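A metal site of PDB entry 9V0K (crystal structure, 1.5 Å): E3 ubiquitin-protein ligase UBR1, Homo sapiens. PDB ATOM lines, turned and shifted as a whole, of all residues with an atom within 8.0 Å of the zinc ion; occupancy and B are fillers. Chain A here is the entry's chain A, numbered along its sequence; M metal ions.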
ATOM      1  N   SER A  17       0.052 -18.282  11.091  1.00  0.00           N
ATOM      2  CA  SER A  17       1.325 -18.731  10.567  1.00  0.00           C
ATOM      3  C   SER A  17       2.434 -18.166  11.439  1.00  0.00           C
ATOM      4  O   SER A  17       2.358 -17.027  11.882  1.00  0.00           O
ATOM      5  CB  SER A  17       1.518 -18.270   9.131  1.00  0.00           C
ATOM      6  OG  SER A  17       1.658 -16.875   9.118  1.00  0.00           O
ATOM      7  N   CYS A  18       3.473 -18.965  11.676  1.00  0.00           N
ATOM      8  CA  CYS A  18       4.606 -18.511  12.437  1.00  0.00           C
ATOM      9  C   CYS A  18       5.711 -18.122  11.472  1.00  0.00           C
ATOM     10  O   CYS A  18       6.260 -18.973  10.775  1.00  0.00           O
ATOM     11  CB  CYS A  18       5.127 -19.571  13.402  1.00  0.00           C
ATOM     12  SG  CYS A  18       6.487 -18.839  14.329  1.00  0.00           S
ATOM     13  N   ARG A  19       6.022 -16.829  11.408  1.00  0.00           N
ATOM     14  CA  ARG A  19       7.053 -16.407  10.473  1.00  0.00           C
ATOM     15  C   ARG A  19       8.443 -16.838  10.943  1.00  0.00           C
ATOM     16  O   ARG A  19       9.319 -17.030  10.114  1.00  0.00           O
ATOM     17  CB  ARG A  19       6.978 -14.898  10.239  1.00  0.00           C
ATOM     18  CG  ARG A  19       5.660 -14.524   9.548  1.00  0.00           C
ATOM     19  CD  ARG A  19       5.599 -13.174   8.950  1.00  0.00           C
ATOM     20  NE  ARG A  19       6.842 -12.646   8.404  1.00  0.00           N
ATOM     21  CZ  ARG A  19       7.270 -12.827   7.155  1.00  0.00           C
ATOM     22  NH1 ARG A  19       6.611 -13.609   6.314  1.00  0.00           N
ATOM     23  NH2 ARG A  19       8.391 -12.231   6.760  1.00  0.00           N
ATOM     24  N   ASP A  20       8.627 -17.080  12.230  1.00  0.00           N
ATOM     25  CA  ASP A  20       9.895 -17.617  12.709  1.00  0.00           C
ATOM     26  C   ASP A  20      10.125 -19.053  12.247  1.00  0.00           C
ATOM     27  O   ASP A  20      11.248 -19.409  11.862  1.00  0.00           O
ATOM     28  CB  ASP A  20       9.968 -17.541  14.233  1.00  0.00           C
ATOM     29  CG  ASP A  20      10.351 -16.158  14.723  1.00  0.00           C
ATOM     30  OD1 ASP A  20      11.371 -15.611  14.244  1.00  0.00           O
ATOM     31  OD2 ASP A  20       9.629 -15.615  15.596  1.00  0.00           O
ATOM     32  N   CYS A  21       9.083 -19.914  12.289  1.00  0.00           N
ATOM     33  CA  CYS A  21       9.261 -21.342  12.142  1.00  0.00           C
ATOM     34  C   CYS A  21       8.680 -21.971  10.879  1.00  0.00           C
ATOM     35  O   CYS A  21       8.988 -23.139  10.607  1.00  0.00           O
ATOM     36  CB  CYS A  21       8.612 -22.082  13.321  1.00  0.00           C
ATOM     37  SG  CYS A  21       9.232 -21.484  14.881  1.00  0.00           S
ATOM     38  N   ALA A  22       7.842 -21.254  10.135  1.00  0.00           N
ATOM     39  CA  ALA A  22       7.219 -21.882   8.965  1.00  0.00           C
ATOM     40  C   ALA A  22       8.272 -22.299   7.939  1.00  0.00           C
ATOM     41  O   ALA A  22       9.165 -21.521   7.605  1.00  0.00           O
ATOM     42  CB  ALA A  22       6.213 -20.926   8.326  1.00  0.00           C
ATOM     43  N   LEU A  29      -1.482 -22.781  11.313  1.00  0.00           N
ATOM     44  CA  LEU A  29      -2.046 -23.479  12.445  1.00  0.00           C
ATOM     45  C   LEU A  29      -3.461 -22.985  12.711  1.00  0.00           C
ATOM     46  O   LEU A  29      -3.764 -21.822  12.466  1.00  0.00           O
ATOM     47  CB  LEU A  29      -1.224 -23.260  13.740  1.00  0.00           C
ATOM     48  CG  LEU A  29       0.227 -23.744  13.666  1.00  0.00           C
ATOM     49  CD1 LEU A  29       1.022 -23.116  14.793  1.00  0.00           C
ATOM     50  CD2 LEU A  29       0.282 -25.264  13.791  1.00  0.00           C
ATOM     51  N   PHE A  34      -2.376 -23.222  17.812  1.00  0.00           N
ATOM     52  CA  PHE A  34      -1.503 -22.064  17.972  1.00  0.00           C
ATOM     53  C   PHE A  34      -1.385 -21.661  19.438  1.00  0.00           C
ATOM     54  O   PHE A  34      -0.268 -21.498  19.945  1.00  0.00           O
ATOM     55  CB  PHE A  34      -2.020 -20.918  17.093  1.00  0.00           C
ATOM     56  CG  PHE A  34      -1.392 -19.620  17.360  1.00  0.00           C
ATOM     57  CD1 PHE A  34      -0.144 -19.317  16.842  1.00  0.00           C
ATOM     58  CD2 PHE A  34      -2.064 -18.653  18.113  1.00  0.00           C
ATOM     59  CE1 PHE A  34       0.432 -18.074  17.082  1.00  0.00           C
ATOM     60  CE2 PHE A  34      -1.490 -17.428  18.331  1.00  0.00           C
ATOM     61  CZ  PHE A  34      -0.247 -17.137  17.824  1.00  0.00           C
ATOM     62  N   SER A  37       0.869 -23.790  21.663  1.00  0.00           N
ATOM     63  CA  SER A  37       2.155 -24.032  21.004  1.00  0.00           C
ATOM     64  C   SER A  37       3.131 -22.919  21.325  1.00  0.00           C
ATOM     65  O   SER A  37       2.779 -21.844  21.813  1.00  0.00           O
ATOM     66  CB  SER A  37       1.995 -24.140  19.463  1.00  0.00           C
ATOM     67  OG  SER A  37       1.900 -22.823  18.884  1.00  0.00           O
ATOM     68  N   VAL A  38       4.396 -23.204  21.023  1.00  0.00           N
ATOM     69  CA  VAL A  38       5.443 -22.224  21.230  1.00  0.00           C
ATOM     70  C   VAL A  38       5.238 -21.006  20.352  1.00  0.00           C
ATOM     71  O   VAL A  38       5.769 -19.928  20.675  1.00  0.00           O
ATOM     72  CB  VAL A  38       6.828 -22.825  20.962  1.00  0.00           C
ATOM     73  CG1 VAL A  38       7.172 -23.890  21.992  1.00  0.00           C
ATOM     74  CG2 VAL A  38       6.924 -23.377  19.554  1.00  0.00           C
ATOM     75  N   HIS A  39       4.532 -21.153  19.231  1.00  0.00           N
ATOM     76  CA  HIS A  39       4.536 -20.100  18.216  1.00  0.00           C
ATOM     77  C   HIS A  39       3.742 -18.861  18.615  1.00  0.00           C
ATOM     78  O   HIS A  39       3.915 -17.816  17.991  1.00  0.00           O
ATOM     79  CB  HIS A  39       4.012 -20.678  16.909  1.00  0.00           C
ATOM     80  CG  HIS A  39       4.713 -21.924  16.511  1.00  0.00           C
ATOM     81  ND1 HIS A  39       6.020 -21.940  16.059  1.00  0.00           N
ATOM     82  CD2 HIS A  39       4.327 -23.220  16.562  1.00  0.00           C
ATOM     83  CE1 HIS A  39       6.380 -23.183  15.810  1.00  0.00           C
ATOM     84  NE2 HIS A  39       5.363 -23.982  16.101  1.00  0.00           N
ATOM     85  N   LYS A  40       2.877 -18.940  19.628  1.00  0.00           N
ATOM     86  CA  LYS A  40       2.237 -17.732  20.146  1.00  0.00           C
ATOM     87  C   LYS A  40       3.225 -16.786  20.804  1.00  0.00           C
ATOM     88  O   LYS A  40       2.898 -15.611  21.027  1.00  0.00           O
ATOM     89  CB  LYS A  40       1.121 -18.075  21.121  1.00  0.00           C
ATOM     90  CG  LYS A  40       1.585 -18.760  22.374  1.00  0.00           C
ATOM     91  CD  LYS A  40       0.389 -19.153  23.219  1.00  0.00           C
ATOM     92  CE  LYS A  40       0.791 -19.757  24.527  1.00  0.00           C
ATOM     93  NZ  LYS A  40      -0.391 -19.872  25.409  1.00  0.00           N
ATOM     94  N   ASN A  41       4.452 -17.256  21.076  1.00  0.00           N
ATOM     95  CA  ASN A  41       5.532 -16.440  21.598  1.00  0.00           C
ATOM     96  C   ASN A  41       6.512 -16.015  20.508  1.00  0.00           C
ATOM     97  O   ASN A  41       7.577 -15.483  20.824  1.00  0.00           O
ATOM     98  CB  ASN A  41       6.261 -17.213  22.703  1.00  0.00           C
ATOM     99  CG  ASN A  41       5.330 -17.573  23.839  1.00  0.00           C
ATOM    100  OD1 ASN A  41       5.236 -18.734  24.279  1.00  0.00           O
ATOM    101  ND2 ASN A  41       4.607 -16.573  24.311  1.00  0.00           N
ATOM    102  N   HIS A  42       6.176 -16.242  19.245  1.00  0.00           N
ATOM    103  CA  HIS A  42       7.049 -15.959  18.119  1.00  0.00           C
ATOM    104  C   HIS A  42       6.441 -14.844  17.269  1.00  0.00           C
ATOM    105  O   HIS A  42       5.404 -14.283  17.593  1.00  0.00           O
ATOM    106  CB  HIS A  42       7.260 -17.215  17.265  1.00  0.00           C
ATOM    107  CG  HIS A  42       7.934 -18.336  17.989  1.00  0.00           C
ATOM    108  ND1 HIS A  42       7.962 -19.624  17.515  1.00  0.00           N
ATOM    109  CD2 HIS A  42       8.566 -18.356  19.186  1.00  0.00           C
ATOM    110  CE1 HIS A  42       8.607 -20.392  18.381  1.00  0.00           C
ATOM    111  NE2 HIS A  42       8.983 -19.638  19.404  1.00  0.00           N
ATOM    112  N   ARG A  43       7.113 -14.520  16.174  1.00  0.00           N
ATOM    113  CA  ARG A  43       6.586 -13.568  15.198  1.00  0.00           C
ATOM    114  C   ARG A  43       5.547 -14.321  14.366  1.00  0.00           C
ATOM    115  O   ARG A  43       5.886 -15.064  13.452  1.00  0.00           O
ATOM    116  CB  ARG A  43       7.707 -13.015  14.326  1.00  0.00           C
ATOM    117  CG  ARG A  43       7.245 -12.069  13.225  1.00  0.00           C
ATOM    118  CD  ARG A  43       6.554 -10.810  13.749  1.00  0.00           C
ATOM    119  NE  ARG A  43       6.991 -10.393  15.072  1.00  0.00           N
ATOM    120  CZ  ARG A  43       6.375  -9.473  15.798  1.00  0.00           C
ATOM    121  NH1 ARG A  43       5.259  -8.891  15.376  1.00  0.00           N
ATOM    122  NH2 ARG A  43       6.876  -9.137  16.983  1.00  0.00           N
ATOM    123  N   TYR A  44       4.289 -14.145  14.702  1.00  0.00           N
ATOM    124  CA  TYR A  44       3.215 -14.811  14.002  1.00  0.00           C
ATOM    125  C   TYR A  44       2.371 -13.814  13.221  1.00  0.00           C
ATOM    126  O   TYR A  44       2.359 -12.615  13.503  1.00  0.00           O
ATOM    127  CB  TYR A  44       2.321 -15.601  14.967  1.00  0.00           C
ATOM    128  CG  TYR A  44       1.534 -14.750  15.929  1.00  0.00           C
ATOM    129  CD1 TYR A  44       0.287 -14.258  15.568  1.00  0.00           C
ATOM    130  CD2 TYR A  44       2.004 -14.490  17.215  1.00  0.00           C
ATOM    131  CE1 TYR A  44      -0.468 -13.526  16.462  1.00  0.00           C
ATOM    132  CE2 TYR A  44       1.248 -13.730  18.104  1.00  0.00           C
ATOM    133  CZ  TYR A  44       0.017 -13.251  17.708  1.00  0.00           C
ATOM    134  OH  TYR A  44      -0.739 -12.509  18.575  1.00  0.00           O
ATOM    135  N   TRP A  63       7.600 -27.298  10.060  1.00  0.00           N
ATOM    136  CA  TRP A  63       8.029 -26.359  11.075  1.00  0.00           C
ATOM    137  C   TRP A  63       9.502 -26.574  11.420  1.00  0.00           C
ATOM    138  O   TRP A  63       9.937 -27.703  11.612  1.00  0.00           O
ATOM    139  CB  TRP A  63       7.202 -26.510  12.355  1.00  0.00           C
ATOM    140  CG  TRP A  63       5.749 -26.376  12.085  1.00  0.00           C
ATOM    141  CD1 TRP A  63       4.829 -27.375  12.025  1.00  0.00           C
ATOM    142  CD2 TRP A  63       5.045 -25.171  11.787  1.00  0.00           C
ATOM    143  NE1 TRP A  63       3.596 -26.879  11.733  1.00  0.00           N
ATOM    144  CE2 TRP A  63       3.712 -25.516  11.565  1.00  0.00           C
ATOM    145  CE3 TRP A  63       5.434 -23.838  11.659  1.00  0.00           C
ATOM    146  CZ2 TRP A  63       2.741 -24.567  11.240  1.00  0.00           C
ATOM    147  CZ3 TRP A  63       4.492 -22.915  11.345  1.00  0.00           C
ATOM    148  CH2 TRP A  63       3.154 -23.273  11.134  1.00  0.00           C
ATOM    149  N   LYS A  64      10.235 -25.470  11.556  1.00  0.00           N
ATOM    150  CA  LYS A  64      11.625 -25.557  11.983  1.00  0.00           C
ATOM    151  C   LYS A  64      11.751 -25.972  13.440  1.00  0.00           C
ATOM    152  O   LYS A  64      12.749 -26.605  13.817  1.00  0.00           O
ATOM    153  CB  LYS A  64      12.323 -24.218  11.755  1.00  0.00           C
ATOM    154  CG  LYS A  64      12.428 -23.783  10.290  1.00  0.00           C
ATOM    155  CD  LYS A  64      13.131 -22.411  10.219  1.00  0.00           C
ATOM    156  CE  LYS A  64      12.411 -21.418   9.327  1.00  0.00           C
ATOM    157  NZ  LYS A  64      13.063 -20.042   9.281  1.00  0.00           N
ATOM    158  N   THR A  65      10.789 -25.595  14.267  1.00  0.00           N
ATOM    159  CA  THR A  65      10.752 -25.886  15.694  1.00  0.00           C
ATOM    160  C   THR A  65       9.291 -26.035  16.058  1.00  0.00           C
ATOM    161  O   THR A  65       8.415 -25.481  15.375  1.00  0.00           O
ATOM    162  CB  THR A  65      11.361 -24.742  16.553  1.00  0.00           C
ATOM    163  OG1 THR A  65      10.344 -23.793  16.888  1.00  0.00           O
ATOM    164  CG2 THR A  65      12.430 -24.033  15.802  1.00  0.00           C
ATOM    165  N   GLY A  66       9.015 -26.746  17.152  1.00  0.00           N
ATOM    166  CA  GLY A  66       7.677 -26.807  17.704  1.00  0.00           C
ATOM    167  C   GLY A  66       6.623 -27.316  16.738  1.00  0.00           C
ATOM    168  O   GLY A  66       5.573 -26.705  16.536  1.00  0.00           O
HETATM  169 ZN    ZN M   1       7.379 -20.414  15.744  1.00  0.00          ZN
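A ring nitrogen (NE2) of His 42 is in hydrogen-bond range of the backbone carbonyl oxygen (O) of Val 38 (3.5 Å). A ring nitrogen (NE2) of His 39 lies close to the backbone carbonyl oxygen of Thr 65, at 3.5 Å. A ring nitrogen (NE2) of His 39 sits at hydrogen-bond distance from the backbone carbonyl oxygen (O) of Gly 66 (2.8 Å). The backbone NH (N) of His 39 sits close to the side-chain hydroxyl (OG) of Ser 37. The backbone NH of Asp 20 lies close to the side-chain sulfur of Cys 18 (3.5 Å). The side-chain hydroxyl of Thr 65 sits close to the side-chain sulfur of Cys 21 (3.3 Å). The backbone NH (N) of Lys 64 is in hydrogen-bond range of the backbone carbonyl oxygen (O) of Cys 21 (2.8 Å).
Four residues have an atom within 4 Å of the zinc ion: Cys 18, Cys 21, His 39 and His 42. Along chain A the residues within 4 Å of the zinc ion span positions 18 to 42.
The zinc ion is bound by ND1 of His 42 (2.0 Å), ND1 of His 39 (2.1 Å), SG of Cys 18 (2.3 Å) and SG of Cys 21 (2.3 Å). The zinc ion has four donor atoms within binding distance.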
